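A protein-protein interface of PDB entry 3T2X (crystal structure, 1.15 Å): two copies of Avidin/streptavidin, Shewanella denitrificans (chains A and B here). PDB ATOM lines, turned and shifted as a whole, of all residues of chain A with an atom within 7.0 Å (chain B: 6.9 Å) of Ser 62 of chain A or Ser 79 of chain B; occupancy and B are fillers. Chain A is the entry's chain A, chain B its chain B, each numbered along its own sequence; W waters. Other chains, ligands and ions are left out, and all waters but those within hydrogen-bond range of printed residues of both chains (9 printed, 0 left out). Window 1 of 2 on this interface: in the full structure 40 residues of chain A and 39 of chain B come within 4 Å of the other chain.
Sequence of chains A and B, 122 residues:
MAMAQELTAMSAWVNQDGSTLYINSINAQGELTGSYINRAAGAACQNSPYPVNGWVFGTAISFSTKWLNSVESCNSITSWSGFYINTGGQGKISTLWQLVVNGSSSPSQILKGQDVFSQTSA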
ATOM      1  N   GLY A  30     -18.342   7.017 -12.031  1.00  0.00           N
ATOM      2  CA  GLY A  30     -19.751   6.885 -12.349  1.00  0.00           C
ATOM      3  C   GLY A  30     -20.110   5.641 -13.119  1.00  0.00           C
ATOM      4  O   GLY A  30     -21.237   5.558 -13.594  1.00  0.00           O
ATOM      5  N   LEU A  32     -21.517   2.040 -13.505  1.00  0.00           N
ATOM      6  CA  LEU A  32     -22.554   1.369 -12.725  1.00  0.00           C
ATOM      7  C   LEU A  32     -22.559  -0.141 -12.971  1.00  0.00           C
ATOM      8  O   LEU A  32     -22.346  -0.597 -14.090  1.00  0.00           O
ATOM      9  CB  LEU A  32     -23.923   2.004 -13.127  1.00  0.00           C
ATOM     10  CG  LEU A  32     -25.257   1.434 -12.681  1.00  0.00           C
ATOM     11  CD1 LEU A  32     -26.293   2.526 -12.749  1.00  0.00           C
ATOM     12  CD2 LEU A  32     -25.696   0.275 -13.538  1.00  0.00           C
ATOM     13  N   VAL A  52     -26.618  -5.882 -15.156  1.00  0.00           N
ATOM     14  CA  VAL A  52     -26.741  -4.517 -15.673  1.00  0.00           C
ATOM     15  C   VAL A  52     -25.404  -3.799 -15.598  1.00  0.00           C
ATOM     16  O   VAL A  52     -24.673  -3.940 -14.610  1.00  0.00           O
ATOM     17  CB  VAL A  52     -27.768  -3.717 -14.828  1.00  0.00           C
ATOM     18  CG1 VAL A  52     -27.937  -2.308 -15.338  1.00  0.00           C
ATOM     19  CG2 VAL A  52     -29.129  -4.429 -14.825  1.00  0.00           C
ATOM     20  N   ASN A  53     -25.094  -3.005 -16.620  1.00  0.00           N
ATOM     21  CA  ASN A  53     -23.984  -2.053 -16.519  1.00  0.00           C
ATOM     22  C   ASN A  53     -24.483  -0.707 -17.060  1.00  0.00           C
ATOM     23  O   ASN A  53     -25.618  -0.594 -17.528  1.00  0.00           O
ATOM     24  CB  ASN A  53     -22.717  -2.585 -17.189  1.00  0.00           C
ATOM     25  CG  ASN A  53     -22.902  -2.895 -18.664  1.00  0.00           C
ATOM     26  OD1 ASN A  53     -23.774  -2.337 -19.332  1.00  0.00           O
ATOM     27  ND2 ASN A  53     -22.065  -3.795 -19.184  1.00  0.00           N
ATOM     28  N   GLY A  54     -23.651   0.314 -16.949  1.00  0.00           N
ATOM     29  CA  GLY A  54     -24.043   1.634 -17.447  1.00  0.00           C
ATOM     30  C   GLY A  54     -23.200   2.717 -16.821  1.00  0.00           C
ATOM     31  O   GLY A  54     -22.070   2.470 -16.368  1.00  0.00           O
ATOM     32  N   TRP A  55     -23.768   3.921 -16.790  1.00  0.00           N
ATOM     33  CA  TRP A  55     -23.051   5.131 -16.370  1.00  0.00           C
ATOM     34  C   TRP A  55     -24.018   6.068 -15.669  1.00  0.00           C
ATOM     35  O   TRP A  55     -25.187   6.183 -16.036  1.00  0.00           O
ATOM     36  CB  TRP A  55     -22.526   5.905 -17.599  1.00  0.00           C
ATOM     37  CG  TRP A  55     -21.475   5.183 -18.375  1.00  0.00           C
ATOM     38  CD1 TRP A  55     -21.628   4.550 -19.566  1.00  0.00           C
ATOM     39  CD2 TRP A  55     -20.111   5.013 -17.996  1.00  0.00           C
ATOM     40  NE1 TRP A  55     -20.434   3.997 -19.973  1.00  0.00           N
ATOM     41  CE2 TRP A  55     -19.474   4.288 -19.035  1.00  0.00           C
ATOM     42  CE3 TRP A  55     -19.342   5.478 -16.916  1.00  0.00           C
ATOM     43  CZ2 TRP A  55     -18.126   3.927 -18.970  1.00  0.00           C
ATOM     44  CZ3 TRP A  55     -18.009   5.126 -16.851  1.00  0.00           C
ATOM     45  CH2 TRP A  55     -17.409   4.370 -17.880  1.00  0.00           C
ATOM     46  N   VAL A  56     -23.451   6.833 -14.739  1.00  0.00           N
ATOM     47  CA  VAL A  56     -24.159   7.974 -14.118  1.00  0.00           C
ATOM     48  C   VAL A  56     -23.310   9.218 -14.319  1.00  0.00           C
ATOM     49  O   VAL A  56     -22.100   9.183 -14.092  1.00  0.00           O
ATOM     50  CB  VAL A  56     -24.403   7.729 -12.630  1.00  0.00           C
ATOM     51  CG1 VAL A  56     -24.985   8.962 -11.951  1.00  0.00           C
ATOM     52  CG2 VAL A  56     -25.332   6.530 -12.460  1.00  0.00           C
ATOM     53  N   PHE A  57     -23.950  10.323 -14.710  1.00  0.00           N
ATOM     54  CA  PHE A  57     -23.263  11.629 -14.842  1.00  0.00           C
ATOM     55  C   PHE A  57     -24.182  12.694 -14.283  1.00  0.00           C
ATOM     56  O   PHE A  57     -25.090  13.180 -14.984  1.00  0.00           O
ATOM     57  CB  PHE A  57     -22.947  11.916 -16.311  1.00  0.00           C
ATOM     58  CG  PHE A  57     -21.959  13.038 -16.561  1.00  0.00           C
ATOM     59  CD1 PHE A  57     -21.622  13.970 -15.562  1.00  0.00           C
ATOM     60  CD2 PHE A  57     -21.367  13.157 -17.810  1.00  0.00           C
ATOM     61  CE1 PHE A  57     -20.700  14.988 -15.824  1.00  0.00           C
ATOM     62  CE2 PHE A  57     -20.432  14.149 -18.064  1.00  0.00           C
ATOM     63  CZ  PHE A  57     -20.109  15.075 -17.091  1.00  0.00           C
ATOM     64  N   ALA A  60     -27.942  12.442 -15.097  1.00  0.00           N
ATOM     65  CA  ALA A  60     -28.088  11.592 -16.289  1.00  0.00           C
ATOM     66  C   ALA A  60     -27.669  10.181 -15.933  1.00  0.00           C
ATOM     67  O   ALA A  60     -26.706   9.980 -15.177  1.00  0.00           O
ATOM     68  CB  ALA A  60     -27.267  12.130 -17.437  1.00  0.00           C
ATOM     69  N   ILE A  61     -28.358   9.200 -16.515  1.00  0.00           N
ATOM     70  CA  ILE A  61     -28.005   7.797 -16.303  1.00  0.00           C
ATOM     71  C   ILE A  61     -28.322   6.995 -17.542  1.00  0.00           C
ATOM     72  O   ILE A  61     -29.335   7.214 -18.196  1.00  0.00           O
ATOM     73  CB  ILE A  61     -28.745   7.193 -15.048  1.00  0.00           C
ATOM     74  CG1 ILE A  61     -28.434   5.717 -14.847  1.00  0.00           C
ATOM     75  CG2 ILE A  61     -30.257   7.492 -15.075  1.00  0.00           C
ATOM     76  CD1 ILE A  61     -28.920   5.117 -13.526  1.00  0.00           C
ATOM     77  N   SER A  62     -27.433   6.064 -17.860  1.00  0.00           N
ATOM     78  CA  SER A  62     -27.764   4.986 -18.793  1.00  0.00           C
ATOM     79  C   SER A  62     -27.562   3.651 -18.104  1.00  0.00           C
ATOM     80  O   SER A  62     -26.655   3.502 -17.281  1.00  0.00           O
ATOM     81  CB  SER A  62     -26.904   5.020 -20.064  1.00  0.00           C
ATOM     82  OG  SER A  62     -25.574   4.585 -19.816  1.00  0.00           O
ATOM     83  N   PHE A  63     -28.407   2.687 -18.437  1.00  0.00           N
ATOM     84  CA  PHE A  63     -28.163   1.318 -17.989  1.00  0.00           C
ATOM     85  C   PHE A  63     -28.673   0.356 -19.024  1.00  0.00           C
ATOM     86  O   PHE A  63     -29.604   0.655 -19.758  1.00  0.00           O
ATOM     87  CB  PHE A  63     -28.717   1.049 -16.575  1.00  0.00           C
ATOM     88  CG  PHE A  63     -30.210   1.300 -16.417  1.00  0.00           C
ATOM     89  CD1 PHE A  63     -30.704   2.563 -16.121  1.00  0.00           C
ATOM     90  CD2 PHE A  63     -31.108   0.248 -16.509  1.00  0.00           C
ATOM     91  CE1 PHE A  63     -32.076   2.792 -15.955  1.00  0.00           C
ATOM     92  CE2 PHE A  63     -32.473   0.456 -16.320  1.00  0.00           C
ATOM     93  CZ  PHE A  63     -32.951   1.728 -16.059  1.00  0.00           C
ATOM     94  N   SER A  64     -28.030  -0.800 -19.072  1.00  0.00           N
ATOM     95  CA  SER A  64     -28.343  -1.790 -20.097  1.00  0.00           C
ATOM     96  C   SER A  64     -28.244  -3.190 -19.515  1.00  0.00           C
ATOM     97  O   SER A  64     -27.339  -3.473 -18.707  1.00  0.00           O
ATOM     98  CB  SER A  64     -27.393  -1.578 -21.299  1.00  0.00           C
ATOM     99  OG  SER A  64     -27.597  -2.537 -22.336  1.00  0.00           O
ATOM    100  N   SER A  79     -31.554  -1.252 -23.498  1.00  0.00           N
ATOM    101  CA  SER A  79     -30.783  -0.098 -23.027  1.00  0.00           C
ATOM    102  C   SER A  79     -31.725   1.016 -22.691  1.00  0.00           C
ATOM    103  O   SER A  79     -32.572   1.398 -23.499  1.00  0.00           O
ATOM    104  CB  SER A  79     -29.854   0.390 -24.126  1.00  0.00           C
ATOM    105  OG  SER A  79     -28.872  -0.588 -24.351  1.00  0.00           O
ATOM    106  N   TRP A  80     -31.555   1.565 -21.499  1.00  0.00           N
ATOM    107  CA  TRP A  80     -32.318   2.710 -21.040  1.00  0.00           C
ATOM    108  C   TRP A  80     -31.418   3.932 -20.969  1.00  0.00           C
ATOM    109  O   TRP A  80     -30.260   3.860 -20.516  1.00  0.00           O
ATOM    110  CB  TRP A  80     -32.850   2.445 -19.622  1.00  0.00           C
ATOM    111  CG  TRP A  80     -33.941   1.410 -19.462  1.00  0.00           C
ATOM    112  CD1 TRP A  80     -35.266   1.654 -19.347  1.00  0.00           C
ATOM    113  CD2 TRP A  80     -33.770  -0.007 -19.329  1.00  0.00           C
ATOM    114  NE1 TRP A  80     -35.956   0.478 -19.128  1.00  0.00           N
ATOM    115  CE2 TRP A  80     -35.048  -0.562 -19.122  1.00  0.00           C
ATOM    116  CE3 TRP A  80     -32.648  -0.851 -19.315  1.00  0.00           C
ATOM    117  CZ2 TRP A  80     -35.234  -1.929 -18.892  1.00  0.00           C
ATOM    118  CZ3 TRP A  80     -32.833  -2.203 -19.091  1.00  0.00           C
ATOM    119  CH2 TRP A  80     -34.116  -2.731 -18.877  1.00  0.00           C
ATOM    120  N   SER A  81     -31.976   5.073 -21.365  1.00  0.00           N
ATOM    121  CA  SER A  81     -31.344   6.384 -21.185  1.00  0.00           C
ATOM    122  C   SER A  81     -32.307   7.237 -20.416  1.00  0.00           C
ATOM    123  O   SER A  81     -33.468   7.299 -20.779  1.00  0.00           O
ATOM    124  CB  SER A  81     -31.080   7.043 -22.530  1.00  0.00           C
ATOM    125  OG  SER A  81     -30.166   6.302 -23.313  1.00  0.00           O
ATOM    126  N   GLY A  82     -31.850   7.903 -19.364  1.00  0.00           N
ATOM    127  CA  GLY A  82     -32.800   8.671 -18.579  1.00  0.00           C
ATOM    128  C   GLY A  82     -32.165   9.657 -17.671  1.00  0.00           C
ATOM    129  O   GLY A  82     -30.936   9.870 -17.643  1.00  0.00           O
ATOM    130  N   GLN A  98     -34.550   1.217 -25.589  1.00  0.00           N
ATOM    131  CA  GLN A  98     -34.463   0.555 -26.885  1.00  0.00           C
ATOM    132  C   GLN A  98     -34.105  -0.900 -26.628  1.00  0.00           C
ATOM    133  O   GLN A  98     -33.252  -1.186 -25.787  1.00  0.00           O
ATOM    134  CB  GLN A  98     -33.377   1.199 -27.731  1.00  0.00           C
ATOM    135  CG  GLN A  98     -33.687   2.676 -28.030  1.00  0.00           C
ATOM    136  CD  GLN A  98     -32.756   3.318 -29.023  1.00  0.00           C
ATOM    137  OE1 GLN A  98     -31.550   3.119 -28.976  1.00  0.00           O
ATOM    138  NE2 GLN A  98     -33.316   4.103 -29.926  1.00  0.00           N
ATOM    139  N   ASN B  53     -18.755   0.853 -22.072  1.00  0.00           N
ATOM    140  CA  ASN B  53     -19.161  -0.463 -21.608  1.00  0.00           C
ATOM    141  C   ASN B  53     -20.399  -0.887 -22.400  1.00  0.00           C
ATOM    142  O   ASN B  53     -20.901  -0.134 -23.223  1.00  0.00           O
ATOM    143  CB  ASN B  53     -19.354  -0.522 -20.091  1.00  0.00           C
ATOM    144  CG  ASN B  53     -20.394   0.468 -19.584  1.00  0.00           C
ATOM    145  OD1 ASN B  53     -21.316   0.871 -20.310  1.00  0.00           O
ATOM    146  ND2 ASN B  53     -20.298   0.814 -18.292  1.00  0.00           N
ATOM    147  N   SER B  62     -25.146  -3.614 -27.437  1.00  0.00           N
ATOM    148  CA  SER B  62     -25.353  -2.271 -26.884  1.00  0.00           C
ATOM    149  C   SER B  62     -24.018  -1.755 -26.385  1.00  0.00           C
ATOM    150  O   SER B  62     -23.180  -2.533 -25.896  1.00  0.00           O
ATOM    151  CB  SER B  62     -26.392  -2.239 -25.758  1.00  0.00           C
ATOM    152  OG  SER B  62     -25.864  -2.813 -24.575  1.00  0.00           O
ATOM    153  N   PHE B  63     -23.810  -0.454 -26.502  1.00  0.00           N
ATOM    154  CA  PHE B  63     -22.638   0.154 -25.862  1.00  0.00           C
ATOM    155  C   PHE B  63     -22.988   1.564 -25.453  1.00  0.00           C
ATOM    156  O   PHE B  63     -23.853   2.197 -26.037  1.00  0.00           O
ATOM    157  CB  PHE B  63     -21.355   0.056 -26.718  1.00  0.00           C
ATOM    158  CG  PHE B  63     -21.443   0.659 -28.100  1.00  0.00           C
ATOM    159  CD1 PHE B  63     -21.978  -0.057 -29.170  1.00  0.00           C
ATOM    160  CD2 PHE B  63     -20.933   1.925 -28.331  1.00  0.00           C
ATOM    161  CE1 PHE B  63     -22.024   0.512 -30.459  1.00  0.00           C
ATOM    162  CE2 PHE B  63     -20.991   2.506 -29.599  1.00  0.00           C
ATOM    163  CZ  PHE B  63     -21.514   1.794 -30.656  1.00  0.00           C
ATOM    164  N   SER B  64     -22.292   2.063 -24.436  1.00  0.00           N
ATOM    165  CA  SER B  64     -22.595   3.376 -23.882  1.00  0.00           C
ATOM    166  C   SER B  64     -21.314   4.038 -23.436  1.00  0.00           C
ATOM    167  O   SER B  64     -20.401   3.375 -22.915  1.00  0.00           O
ATOM    168  CB  SER B  64     -23.557   3.206 -22.721  1.00  0.00           C
ATOM    169  OG  SER B  64     -23.947   4.455 -22.145  1.00  0.00           O
ATOM    170  N   THR B  65     -21.261   5.356 -23.602  1.00  0.00           N
ATOM    171  CA  THR B  65     -20.124   6.158 -23.158  1.00  0.00           C
ATOM    172  C   THR B  65     -20.610   7.358 -22.372  1.00  0.00           C
ATOM    173  O   THR B  65     -21.560   8.023 -22.764  1.00  0.00           O
ATOM    174  CB  THR B  65     -19.204   6.577 -24.319  1.00  0.00           C
ATOM    175  OG1 THR B  65     -17.948   7.030 -23.791  1.00  0.00           O
ATOM    176  CG2 THR B  65     -19.764   7.685 -25.184  1.00  0.00           C
ATOM    177  N   LYS B  66     -19.943   7.614 -21.250  1.00  0.00           N
ATOM    178  CA  LYS B  66     -20.114   8.849 -20.493  1.00  0.00           C
ATOM    179  C   LYS B  66     -19.118   9.890 -21.015  1.00  0.00           C
ATOM    180  O   LYS B  66     -17.916   9.606 -21.073  1.00  0.00           O
ATOM    181  CB  LYS B  66     -19.887   8.538 -19.001  1.00  0.00           C
ATOM    182  CG  LYS B  66     -19.786   9.780 -18.117  1.00  0.00           C
ATOM    183  CD  LYS B  66     -19.717   9.393 -16.632  1.00  0.00           C
ATOM    184  CE  LYS B  66     -19.433  10.629 -15.762  1.00  0.00           C
ATOM    185  NZ  LYS B  66     -19.495  10.268 -14.331  1.00  0.00           N
ATOM    186  N   TRP B  67     -19.598  11.091 -21.358  1.00  0.00           N
ATOM    187  CA  TRP B  67     -18.726  12.054 -21.984  1.00  0.00           C
ATOM    188  C   TRP B  67     -17.994  12.871 -20.907  1.00  0.00           C
ATOM    189  O   TRP B  67     -18.178  14.086 -20.788  1.00  0.00           O
ATOM    190  CB  TRP B  67     -19.521  12.976 -22.911  1.00  0.00           C
ATOM    191  CG  TRP B  67     -20.121  12.252 -24.071  1.00  0.00           C
ATOM    192  CD1 TRP B  67     -21.434  11.898 -24.238  1.00  0.00           C
ATOM    193  CD2 TRP B  67     -19.429  11.803 -25.228  1.00  0.00           C
ATOM    194  NE1 TRP B  67     -21.597  11.250 -25.445  1.00  0.00           N
ATOM    195  CE2 TRP B  67     -20.373  11.178 -26.054  1.00  0.00           C
ATOM    196  CE3 TRP B  67     -18.091  11.849 -25.640  1.00  0.00           C
ATOM    197  CZ2 TRP B  67     -20.028  10.634 -27.279  1.00  0.00           C
ATOM    198  CZ3 TRP B  67     -17.746  11.285 -26.858  1.00  0.00           C
ATOM    199  CH2 TRP B  67     -18.705  10.677 -27.655  1.00  0.00           C
ATOM    200  N   ILE B  77     -24.415  11.462 -21.652  1.00  0.00           N
ATOM    201  CA  ILE B  77     -24.140  10.038 -21.852  1.00  0.00           C
ATOM    202  C   ILE B  77     -24.849   9.636 -23.130  1.00  0.00           C
ATOM    203  O   ILE B  77     -26.019   9.946 -23.337  1.00  0.00           O
ATOM    204  CB  ILE B  77     -24.687   9.174 -20.699  1.00  0.00           C
ATOM    205  CG1 ILE B  77     -24.077   9.610 -19.358  1.00  0.00           C
ATOM    206  CG2 ILE B  77     -24.423   7.669 -20.978  1.00  0.00           C
ATOM    207  CD1 ILE B  77     -24.867   9.014 -18.189  1.00  0.00           C
ATOM    208  N   THR B  78     -24.120   8.957 -24.007  1.00  0.00           N
ATOM    209  CA  THR B  78     -24.718   8.365 -25.218  1.00  0.00           C
ATOM    210  C   THR B  78     -24.804   6.872 -25.074  1.00  0.00           C
ATOM    211  O   THR B  78     -23.867   6.201 -24.610  1.00  0.00           O
ATOM    212  CB  THR B  78     -23.939   8.748 -26.503  1.00  0.00           C
ATOM    213  OG1 THR B  78     -23.930  10.176 -26.599  1.00  0.00           O
ATOM    214  CG2 THR B  78     -24.555   8.127 -27.770  1.00  0.00           C
ATOM    215  N   SER B  79     -25.925   6.314 -25.511  1.00  0.00           N
ATOM    216  CA  SER B  79     -26.150   4.854 -25.545  1.00  0.00           C
ATOM    217  C   SER B  79     -26.594   4.442 -26.911  1.00  0.00           C
ATOM    218  O   SER B  79     -27.536   5.006 -27.460  1.00  0.00           O
ATOM    219  CB  SER B  79     -27.231   4.487 -24.551  1.00  0.00           C
ATOM    220  OG  SER B  79     -26.811   4.791 -23.233  1.00  0.00           O
ATOM    221  N   TRP B  80     -25.901   3.444 -27.442  1.00  0.00           N
ATOM    222  CA  TRP B  80     -26.212   2.860 -28.732  1.00  0.00           C
ATOM    223  C   TRP B  80     -26.793   1.467 -28.557  1.00  0.00           C
ATOM    224  O   TRP B  80     -26.338   0.669 -27.713  1.00  0.00           O
ATOM    225  CB  TRP B  80     -24.958   2.710 -29.571  1.00  0.00           C
ATOM    226  CG  TRP B  80     -24.251   3.961 -30.049  1.00  0.00           C
ATOM    227  CD1 TRP B  80     -24.333   4.496 -31.303  1.00  0.00           C
ATOM    228  CD2 TRP B  80     -23.324   4.794 -29.311  1.00  0.00           C
ATOM    229  NE1 TRP B  80     -23.493   5.578 -31.408  1.00  0.00           N
ATOM    230  CE2 TRP B  80     -22.860   5.777 -30.204  1.00  0.00           C
ATOM    231  CE3 TRP B  80     -22.791   4.759 -28.003  1.00  0.00           C
ATOM    232  CZ2 TRP B  80     -21.888   6.731 -29.842  1.00  0.00           C
ATOM    233  CZ3 TRP B  80     -21.821   5.691 -27.646  1.00  0.00           C
ATOM    234  CH2 TRP B  80     -21.384   6.667 -28.565  1.00  0.00           C
ATOM    235  N   SER B  81     -27.797   1.146 -29.377  1.00  0.00           N
ATOM    236  CA  SER B  81     -28.352  -0.196 -29.511  1.00  0.00           C
ATOM    237  C   SER B  81     -28.269  -0.564 -30.960  1.00  0.00           C
ATOM    238  O   SER B  81     -28.708   0.193 -31.816  1.00  0.00           O
ATOM    239  CB  SER B  81     -29.816  -0.225 -29.074  1.00  0.00           C
ATOM    240  OG  SER B  81     -29.959   0.129 -27.722  1.00  0.00           O
ATOM    241  N   LEU B  96     -29.088   2.565 -33.430  1.00  0.00           N
ATOM    242  CA  LEU B  96     -29.841   3.748 -33.012  1.00  0.00           C
ATOM    243  C   LEU B  96     -29.211   4.202 -31.726  1.00  0.00           C
ATOM    244  O   LEU B  96     -28.776   3.380 -30.914  1.00  0.00           O
ATOM    245  CB  LEU B  96     -31.331   3.437 -32.780  1.00  0.00           C
ATOM    246  CG  LEU B  96     -32.091   2.905 -33.993  1.00  0.00           C
ATOM    247  CD1 LEU B  96     -33.533   2.653 -33.612  1.00  0.00           C
ATOM    248  CD2 LEU B  96     -32.060   3.880 -35.158  1.00  0.00           C
ATOM    249  N   TRP B  97     -29.169   5.504 -31.500  1.00  0.00           N
ATOM    250  CA  TRP B  97     -28.614   5.992 -30.246  1.00  0.00           C
ATOM    251  C   TRP B  97     -29.514   7.024 -29.580  1.00  0.00           C
ATOM    252  O   TRP B  97     -30.381   7.649 -30.217  1.00  0.00           O
ATOM    253  CB  TRP B  97     -27.186   6.554 -30.389  1.00  0.00           C
ATOM    254  CG  TRP B  97     -27.024   7.684 -31.381  1.00  0.00           C
ATOM    255  CD1 TRP B  97     -26.531   7.570 -32.627  1.00  0.00           C
ATOM    256  CD2 TRP B  97     -27.370   9.080 -31.195  1.00  0.00           C
ATOM    257  NE1 TRP B  97     -26.527   8.799 -33.241  1.00  0.00           N
ATOM    258  CE2 TRP B  97     -27.042   9.744 -32.393  1.00  0.00           C
ATOM    259  CE3 TRP B  97     -27.889   9.830 -30.118  1.00  0.00           C
ATOM    260  CZ2 TRP B  97     -27.217  11.121 -32.572  1.00  0.00           C
ATOM    261  CZ3 TRP B  97     -28.078  11.224 -30.296  1.00  0.00           C
ATOM    262  CH2 TRP B  97     -27.745  11.834 -31.518  1.00  0.00           C
ATOM    263  N   GLN B  98     -29.305   7.167 -28.273  1.00  0.00           N
ATOM    264  CA  GLN B  98     -29.957   8.183 -27.438  1.00  0.00           C
ATOM    265  C   GLN B  98     -28.889   8.871 -26.637  1.00  0.00           C
ATOM    266  O   GLN B  98     -27.981   8.223 -26.116  1.00  0.00           O
ATOM    267  CB  GLN B  98     -30.990   7.553 -26.517  1.00  0.00           C
ATOM    268  CG  GLN B  98     -32.082   6.854 -27.304  1.00  0.00           C
ATOM    269  CD  GLN B  98     -33.146   6.238 -26.450  1.00  0.00           C
ATOM    270  OE1 GLN B  98     -32.880   5.610 -25.416  1.00  0.00           O
ATOM    271  NE2 GLN B  98     -34.370   6.402 -26.877  1.00  0.00           N
ATOM    272  N   LEU B  99     -29.042  10.187 -26.500  1.00  0.00           N
ATOM    273  CA  LEU B  99     -28.127  11.041 -25.752  1.00  0.00           C
ATOM    274  C   LEU B  99     -28.904  11.732 -24.646  1.00  0.00           C
ATOM    275  O   LEU B  99     -29.838  12.463 -24.957  1.00  0.00           O
ATOM    276  CB  LEU B  99     -27.521  12.064 -26.716  1.00  0.00           C
ATOM    277  CG  LEU B  99     -26.646  13.215 -26.199  1.00  0.00           C
ATOM    278  CD1 LEU B  99     -27.414  14.359 -25.523  1.00  0.00           C
ATOM    279  CD2 LEU B  99     -25.505  12.735 -25.327  1.00  0.00           C
ATOM    280  N   VAL B 100     -28.507  11.519 -23.386  1.00  0.00           N
ATOM    281  CA  VAL B 100     -29.145  12.200 -22.264  1.00  0.00           C
ATOM    282  C   VAL B 100     -28.163  13.152 -21.623  1.00  0.00           C
ATOM    283  O   VAL B 100     -27.011  12.809 -21.342  1.00  0.00           O
ATOM    284  CB  VAL B 100     -29.796  11.215 -21.255  1.00  0.00           C
ATOM    285  CG1 VAL B 100     -28.806  10.226 -20.645  1.00  0.00           C
ATOM    286  CG2 VAL B 100     -30.540  11.985 -20.184  1.00  0.00           C
HETATM  287  O   HOH W   1     -29.798   2.861 -26.876  1.00  0.00           O
HETATM  288  O   HOH W   2     -30.949   3.921 -24.609  1.00  0.00           O
HETATM  289  O   HOH W   3     -29.991  -2.212 -26.387  1.00  0.00           O
HETATM  290  O   HOH W   4     -28.108   2.457 -22.043  1.00  0.00           O
HETATM  291  O   HOH W   5     -32.756   6.514 -31.373  1.00  0.00           O
HETATM  292  O   HOH W   6     -23.884   0.010 -20.819  1.00  0.00           O
HETATM  293  O   HOH W   7     -26.632   1.125 -24.779  1.00  0.00           O
HETATM  294  O   HOH W   8     -20.211  10.030 -11.277  1.00  0.00           O
HETATM  295  O   HOH W   9     -27.743   7.402 -22.841  1.00  0.00           O
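Of the 17 printed residues of chain B, 12 touch a printed residue of chain A. Printed residues of chain B that touch a printed residue of chain A: Asn 53, Ser 62, Ser 64, Thr 65, Lys 66, Trp 67, Ile 77, Ser 79, Ser 81, Leu 96, Gln 98 and Val 100. Among the printed residues, no Asp or Glu carboxylate lies within 4 Å of a Lys or Arg side-chain nitrogen of the other chain.
Of the printed residues of chain B, Ser 62 of chain A touches Ser 64 (2.8 Å), Ile 77 (3.5 Å) and Ser 79 (3.2 Å). Printed residues of chain A within 4 Å of Ser 62 of chain B: Ser 64 (2.8 Å) and Ser 79 (3.3 Å). Of the printed residues of chain B, Ser 79 of chain A touches Ser 62 (3.3 Å) and Ser 81 (3.6 Å). The nearest printed residue of chain A that does not touch Ser 79 of chain B is Trp 80 of chain A (4.5 Å).
Among the printed residues, pairs that only touch across the chains: Gly 30 of chain A with Lys 66 of chain B (3.9 Å), Trp 55 of chain A with Thr 65 of chain B (3.9 Å), Trp 55 of chain A with Lys 66 of chain B (3.7 Å), Trp 55 of chain A with Ile 77 of chain B (3.6 Å), Phe 57 of chain A with Lys 66 of chain B (3.6 Å), Phe 57 of chain A with Trp 67 of chain B (3.5 Å), Phe 57 of chain A with Ile 77 of chain B (3.8 Å), Ala 60 of chain A with Ile 77 of chain B (3.7 Å), Ala 60 of chain A with Val 100 of chain B (3.97 Å), Ile 61 of chain A with Ile 77 of chain B (3.9 Å), Ile 61 of chain A with Val 100 of chain B (3.9 Å), Ser 62 of chain A with Ile 77 of chain B (3.5 Å), Ser 62 of chain A with Ser 79 of chain B (3.2 Å), Ser 79 of chain A with Ser 62 of chain B (3.3 Å), Ser 79 of chain A with Ser 81 of chain B (3.6 Å), Ser 81 of chain A with Ser 79 of chain B (3.7 Å), Ser 81 of chain A with Gln 98 of chain B (3.5 Å), Gly 82 of chain A with Val 100 of chain B (3.3 Å), Gln 98 of chain A with Ser 81 of chain B (3.6 Å) and Gln 98 of chain A with Gln 98 of chain B (3.9 Å).
Water W7 lies within hydrogen-bond range of OG of Ser 79 of chain A (2.9 Å), O of Trp 80 of chain B (3.0 Å) and O of Phe 63 of chain B (3.2 Å). Water W5 lies within hydrogen-bond range of NE2 of Gln 98 of chain A and O of Trp 97 of chain B. Water W8 bridges NZ of Lys 66 of chain B and O of Val 56 of chain A.
The backbone carbonyl oxygen (O) of Gly 30 of chain A lies within hydrogen-bond range of the backbone NH (N) of Val 56 of chain A, at 2.8 Å. The side-chain hydroxyl (OG) of Ser 64 of chain B sits at hydrogen-bond distance from the backbone carbonyl oxygen (O) of Thr 78 of chain B (3.0 Å). O of Val 100 of chain B is in hydrogen-bond range of N of Ile 77 of chain B, at 2.9 Å.
Ser 62 of chain A touches Ser 79 of chain B, and with the chains exchanged Ser 79 of chain A touches Ser 62 of chain B. Gln 98 of chain B touches its own counterpart, Gln 98 of chain A. Of the 27 pairs that touch across the chains among the printed residues, 9 have their exchanged pair printed and touching as well.
The backbone carbonyl oxygen (O) of Gly 54 of chain A is in hydrogen-bond range of the side-chain amide nitrogen (ND2) of Asn 53 of chain B (3.1 Å). The indole nitrogen (NE1) of Trp 55 of chain A sits at hydrogen-bond distance from the side-chain amide oxygen (OD1) of Asn 53 of chain B. NE1 of Trp 55 of chain A lies within hydrogen-bond range of O of Ser 64 of chain B (3.0 Å). O of Val 56 of chain A lies within hydrogen-bond range of NZ of Lys 66 of chain B, at 2.8 Å. OG of Ser 64 of chain B sits at hydrogen-bond distance from OG of Ser 62 of chain A, at 2.8 Å. The side-chain hydroxyl of Ser 64 of chain A is in hydrogen-bond range of the side-chain hydroxyl of Ser 62 of chain B, at 2.8 Å. The side-chain amide oxygen (OE1) of Gln 98 of chain A sits close to the backbone carbonyl oxygen (O) of Leu 96 of chain B (3.4 Å).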
